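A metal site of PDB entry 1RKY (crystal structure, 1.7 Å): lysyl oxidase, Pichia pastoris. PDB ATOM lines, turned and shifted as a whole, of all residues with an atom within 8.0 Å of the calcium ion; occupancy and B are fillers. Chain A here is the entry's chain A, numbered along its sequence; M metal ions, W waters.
OE2 of Glu 540 sits close to N of Lys 606, 2.9 Å away.
The side-chain carboxylate (OE2) of Glu 637 is in salt-bridge range of the side-chain amino group (NZ) of Lys 608, at 2.8 Å.
The backbone NH (N) of Asp 636 sits close to the side-chain carboxylate (OE1) of Glu 540.
Four residues have an atom within 4 Å of the calcium ion: Glu 540, Phe 633, Asp 635 and Glu 637.
The calcium ion is bound by water W1, 2.3 Å away.
OE1 of Glu 637 is bound to the calcium ion, at 2.3 Å.
The backbone carbonyl oxygen (O) of Phe 633 is bound to the calcium ion (2.4 Å).
Water W2 binds the calcium ion (2.4 Å).
The side-chain carboxylate (OD2) of Asp 635 is bound to the calcium ion (2.4 Å).
OE2 of Glu 540 is bound to the calcium ion (2.5 Å).
The calcium ion is bound by OE1 of Glu 540 (2.5 Å).
The calcium ion has seven donor atoms within binding distance.
Water W1 lies within hydrogen-bond range of OD1 of Asp 635 (2.7 Å), OE2 of Glu 611 (2.7 Å) and NZ of Lys 608 (3.0 Å).
Water W2 lies within hydrogen-bond range of the side-chain carboxylate (OE1) of Glu 611 (2.6 Å) and the backbone carbonyl oxygen (O) of Lys 606 (2.8 Å).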
ATOM      1  N   GLU A 540       2.451  21.242 -30.576  1.00  0.00           N
ATOM      2  CA  GLU A 540       1.416  22.228 -30.803  1.00  0.00           C
ATOM      3  C   GLU A 540       1.042  22.186 -32.277  1.00  0.00           C
ATOM      4  O   GLU A 540       1.909  22.184 -33.143  1.00  0.00           O
ATOM      5  CB  GLU A 540       1.893  23.638 -30.464  1.00  0.00           C
ATOM      6  CG  GLU A 540       2.123  23.791 -28.982  1.00  0.00           C
ATOM      7  CD  GLU A 540       2.751  25.104 -28.602  1.00  0.00           C
ATOM      8  OE1 GLU A 540       3.462  25.683 -29.456  1.00  0.00           O
ATOM      9  OE2 GLU A 540       2.576  25.531 -27.434  1.00  0.00           O
ATOM     10  N   LEU A 604      -4.201  23.118 -28.036  1.00  0.00           N
ATOM     11  CA  LEU A 604      -3.357  22.682 -26.934  1.00  0.00           C
ATOM     12  C   LEU A 604      -2.026  23.398 -27.078  1.00  0.00           C
ATOM     13  O   LEU A 604      -1.428  23.430 -28.146  1.00  0.00           O
ATOM     14  CB  LEU A 604      -3.141  21.178 -26.952  1.00  0.00           C
ATOM     15  CG  LEU A 604      -4.365  20.284 -26.929  1.00  0.00           C
ATOM     16  CD1 LEU A 604      -3.987  18.839 -27.165  1.00  0.00           C
ATOM     17  CD2 LEU A 604      -5.103  20.430 -25.630  1.00  0.00           C
ATOM     18  N   THR A 605      -1.614  24.047 -26.006  1.00  0.00           N
ATOM     19  CA  THR A 605      -0.355  24.801 -25.988  1.00  0.00           C
ATOM     20  C   THR A 605       0.433  24.463 -24.746  1.00  0.00           C
ATOM     21  O   THR A 605      -0.112  23.940 -23.751  1.00  0.00           O
ATOM     22  CB  THR A 605      -0.581  26.338 -26.039  1.00  0.00           C
ATOM     23  OG1 THR A 605      -1.231  26.797 -24.852  1.00  0.00           O
ATOM     24  CG2 THR A 605      -1.454  26.766 -27.192  1.00  0.00           C
ATOM     25  N   LYS A 606       1.726  24.776 -24.796  1.00  0.00           N
ATOM     26  CA  LYS A 606       2.596  24.685 -23.637  1.00  0.00           C
ATOM     27  C   LYS A 606       2.354  25.911 -22.784  1.00  0.00           C
ATOM     28  O   LYS A 606       2.370  27.051 -23.265  1.00  0.00           O
ATOM     29  CB  LYS A 606       4.060  24.635 -24.091  1.00  0.00           C
ATOM     30  CG  LYS A 606       5.086  24.777 -22.994  1.00  0.00           C
ATOM     31  CD  LYS A 606       6.492  24.564 -23.597  1.00  0.00           C
ATOM     32  CE  LYS A 606       7.595  25.048 -22.657  1.00  0.00           C
ATOM     33  NZ  LYS A 606       8.944  24.870 -23.285  1.00  0.00           N
ATOM     34  N   HIS A 607       2.108  25.674 -21.501  1.00  0.00           N
ATOM     35  CA  HIS A 607       1.840  26.747 -20.571  1.00  0.00           C
ATOM     36  C   HIS A 607       2.993  27.723 -20.506  1.00  0.00           C
ATOM     37  O   HIS A 607       4.166  27.317 -20.449  1.00  0.00           O
ATOM     38  CB  HIS A 607       1.608  26.210 -19.155  1.00  0.00           C
ATOM     39  CG  HIS A 607       1.306  27.297 -18.189  1.00  0.00           C
ATOM     40  ND1 HIS A 607       2.298  28.043 -17.580  1.00  0.00           N
ATOM     41  CD2 HIS A 607       0.123  27.858 -17.824  1.00  0.00           C
ATOM     42  CE1 HIS A 607       1.731  28.998 -16.858  1.00  0.00           C
ATOM     43  NE2 HIS A 607       0.421  28.902 -16.977  1.00  0.00           N
ATOM     44  N   LYS A 608       2.675  29.002 -20.559  1.00  0.00           N
ATOM     45  CA  LYS A 608       3.632  30.098 -20.368  1.00  0.00           C
ATOM     46  C   LYS A 608       2.956  31.239 -19.618  1.00  0.00           C
ATOM     47  O   LYS A 608       1.818  31.591 -19.915  1.00  0.00           O
ATOM     48  CB  LYS A 608       4.124  30.623 -21.694  1.00  0.00           C
ATOM     49  CG  LYS A 608       5.014  29.672 -22.431  1.00  0.00           C
ATOM     50  CD  LYS A 608       5.427  30.164 -23.786  1.00  0.00           C
ATOM     51  CE  LYS A 608       6.317  29.113 -24.462  1.00  0.00           C
ATOM     52  NZ  LYS A 608       6.805  29.612 -25.764  1.00  0.00           N
ATOM     53  N   GLU A 611       1.753  33.768 -21.921  1.00  0.00           N
ATOM     54  CA  GLU A 611       0.531  33.444 -22.639  1.00  0.00           C
ATOM     55  C   GLU A 611      -0.592  33.255 -21.635  1.00  0.00           C
ATOM     56  O   GLU A 611      -1.187  32.183 -21.454  1.00  0.00           O
ATOM     57  CB  GLU A 611       0.780  32.228 -23.536  1.00  0.00           C
ATOM     58  CG  GLU A 611       1.962  32.534 -24.455  1.00  0.00           C
ATOM     59  CD  GLU A 611       2.279  31.471 -25.463  1.00  0.00           C
ATOM     60  OE1 GLU A 611       1.696  30.362 -25.396  1.00  0.00           O
ATOM     61  OE2 GLU A 611       3.162  31.744 -26.325  1.00  0.00           O
ATOM     62  N   PHE A 630      -3.483  35.358 -30.818  1.00  0.00           N
ATOM     63  CA  PHE A 630      -3.461  33.990 -30.317  1.00  0.00           C
ATOM     64  C   PHE A 630      -2.556  33.057 -31.118  1.00  0.00           C
ATOM     65  O   PHE A 630      -2.001  32.123 -30.578  1.00  0.00           O
ATOM     66  CB  PHE A 630      -4.888  33.449 -30.321  1.00  0.00           C
ATOM     67  CG  PHE A 630      -4.994  32.037 -29.816  1.00  0.00           C
ATOM     68  CD1 PHE A 630      -4.968  31.757 -28.444  1.00  0.00           C
ATOM     69  CD2 PHE A 630      -5.086  30.992 -30.698  1.00  0.00           C
ATOM     70  CE1 PHE A 630      -5.011  30.472 -27.980  1.00  0.00           C
ATOM     71  CE2 PHE A 630      -5.176  29.667 -30.231  1.00  0.00           C
ATOM     72  CZ  PHE A 630      -5.152  29.420 -28.853  1.00  0.00           C
ATOM     73  N   ASN A 631      -2.459  33.292 -32.427  1.00  0.00           N
ATOM     74  CA  ASN A 631      -1.603  32.475 -33.272  1.00  0.00           C
ATOM     75  C   ASN A 631      -0.148  32.493 -32.864  1.00  0.00           C
ATOM     76  O   ASN A 631       0.575  31.515 -33.125  1.00  0.00           O
ATOM     77  CB  ASN A 631      -1.766  32.840 -34.746  1.00  0.00           C
ATOM     78  CG  ASN A 631      -3.062  32.347 -35.331  1.00  0.00           C
ATOM     79  OD1 ASN A 631      -3.770  31.542 -34.709  1.00  0.00           O
ATOM     80  ND2 ASN A 631      -3.378  32.811 -36.546  1.00  0.00           N
ATOM     81  N   ALA A 632       0.280  33.527 -32.152  1.00  0.00           N
ATOM     82  CA  ALA A 632       1.648  33.567 -31.634  1.00  0.00           C
ATOM     83  C   ALA A 632       1.942  32.457 -30.637  1.00  0.00           C
ATOM     84  O   ALA A 632       3.086  32.102 -30.441  1.00  0.00           O
ATOM     85  CB  ALA A 632       1.939  34.920 -31.009  1.00  0.00           C
ATOM     86  N   PHE A 633       0.931  31.907 -29.991  1.00  0.00           N
ATOM     87  CA  PHE A 633       1.105  30.805 -29.039  1.00  0.00           C
ATOM     88  C   PHE A 633       1.498  29.491 -29.725  1.00  0.00           C
ATOM     89  O   PHE A 633       1.992  28.591 -29.086  1.00  0.00           O
ATOM     90  CB  PHE A 633      -0.198  30.493 -28.268  1.00  0.00           C
ATOM     91  CG  PHE A 633      -0.746  31.607 -27.385  1.00  0.00           C
ATOM     92  CD1 PHE A 633      -0.186  32.879 -27.326  1.00  0.00           C
ATOM     93  CD2 PHE A 633      -1.880  31.339 -26.606  1.00  0.00           C
ATOM     94  CE1 PHE A 633      -0.758  33.878 -26.510  1.00  0.00           C
ATOM     95  CE2 PHE A 633      -2.448  32.318 -25.785  1.00  0.00           C
ATOM     96  CZ  PHE A 633      -1.885  33.599 -25.737  1.00  0.00           C
ATOM     97  N   LEU A 634       1.176  29.391 -31.012  1.00  0.00           N
ATOM     98  CA  LEU A 634       1.226  28.165 -31.764  1.00  0.00           C
ATOM     99  C   LEU A 634       2.495  28.148 -32.610  1.00  0.00           C
ATOM    100  O   LEU A 634       2.522  28.627 -33.728  1.00  0.00           O
ATOM    101  CB  LEU A 634      -0.005  28.059 -32.646  1.00  0.00           C
ATOM    102  CG  LEU A 634      -1.338  28.079 -31.905  1.00  0.00           C
ATOM    103  CD1 LEU A 634      -2.455  28.272 -32.894  1.00  0.00           C
ATOM    104  CD2 LEU A 634      -1.504  26.810 -31.120  1.00  0.00           C
ATOM    105  N   ASP A 635       3.537  27.598 -32.027  1.00  0.00           N
ATOM    106  CA  ASP A 635       4.881  27.638 -32.620  1.00  0.00           C
ATOM    107  C   ASP A 635       5.568  26.281 -32.488  1.00  0.00           C
ATOM    108  O   ASP A 635       6.800  26.162 -32.335  1.00  0.00           O
ATOM    109  CB  ASP A 635       5.703  28.809 -32.030  1.00  0.00           C
ATOM    110  CG  ASP A 635       5.634  28.902 -30.523  1.00  0.00           C
ATOM    111  OD1 ASP A 635       5.948  29.991 -29.963  1.00  0.00           O
ATOM    112  OD2 ASP A 635       5.306  27.962 -29.807  1.00  0.00           O
ATOM    113  N   ASP A 636       4.756  25.235 -32.583  1.00  0.00           N
ATOM    114  CA  ASP A 636       5.229  23.871 -32.777  1.00  0.00           C
ATOM    115  C   ASP A 636       6.037  23.307 -31.618  1.00  0.00           C
ATOM    116  O   ASP A 636       6.865  22.425 -31.823  1.00  0.00           O
ATOM    117  CB  ASP A 636       6.050  23.784 -34.072  1.00  0.00           C
ATOM    118  CG  ASP A 636       6.302  22.369 -34.511  1.00  0.00           C
ATOM    119  OD1 ASP A 636       5.361  21.540 -34.443  1.00  0.00           O
ATOM    120  OD2 ASP A 636       7.429  21.985 -34.921  1.00  0.00           O
ATOM    121  N   GLU A 637       5.798  23.832 -30.431  1.00  0.00           N
ATOM    122  CA  GLU A 637       6.502  23.338 -29.248  1.00  0.00           C
ATOM    123  C   GLU A 637       6.075  21.947 -28.880  1.00  0.00           C
ATOM    124  O   GLU A 637       4.928  21.541 -29.058  1.00  0.00           O
ATOM    125  CB  GLU A 637       6.406  24.285 -28.076  1.00  0.00           C
ATOM    126  CG  GLU A 637       7.119  25.604 -28.319  1.00  0.00           C
ATOM    127  CD  GLU A 637       6.906  26.644 -27.227  1.00  0.00           C
ATOM    128  OE1 GLU A 637       5.741  26.945 -26.872  1.00  0.00           O
ATOM    129  OE2 GLU A 637       7.919  27.192 -26.717  1.00  0.00           O
ATOM    130  N   SER A 638       7.019  21.170 -28.376  1.00  0.00           N
ATOM    131  CA  SER A 638       6.695  19.854 -27.869  1.00  0.00           C
ATOM    132  C   SER A 638       5.677  19.901 -26.713  1.00  0.00           C
ATOM    133  O   SER A 638       5.778  20.733 -25.807  1.00  0.00           O
ATOM    134  CB  SER A 638       7.953  19.106 -27.402  1.00  0.00           C
ATOM    135  OG  SER A 638       7.591  17.821 -26.908  1.00  0.00           O
ATOM    136  N   LEU A 639       4.672  19.029 -26.767  1.00  0.00           N
ATOM    137  CA  LEU A 639       3.740  18.816 -25.664  1.00  0.00           C
ATOM    138  C   LEU A 639       3.961  17.474 -24.997  1.00  0.00           C
ATOM    139  O   LEU A 639       3.172  17.045 -24.198  1.00  0.00           O
ATOM    140  CB  LEU A 639       2.303  18.875 -26.154  1.00  0.00           C
ATOM    141  CG  LEU A 639       1.925  20.156 -26.865  1.00  0.00           C
ATOM    142  CD1 LEU A 639       0.554  19.991 -27.504  1.00  0.00           C
ATOM    143  CD2 LEU A 639       1.911  21.356 -25.915  1.00  0.00           C
HETATM  144 CA    CA M   1       3.829  27.663 -27.933  1.00  0.00          CA
HETATM  145  O   HOH W   1       4.503  29.821 -27.685  1.00  0.00           O
HETATM  146  O   HOH W   2       2.988  28.160 -25.738  1.00  0.00           O
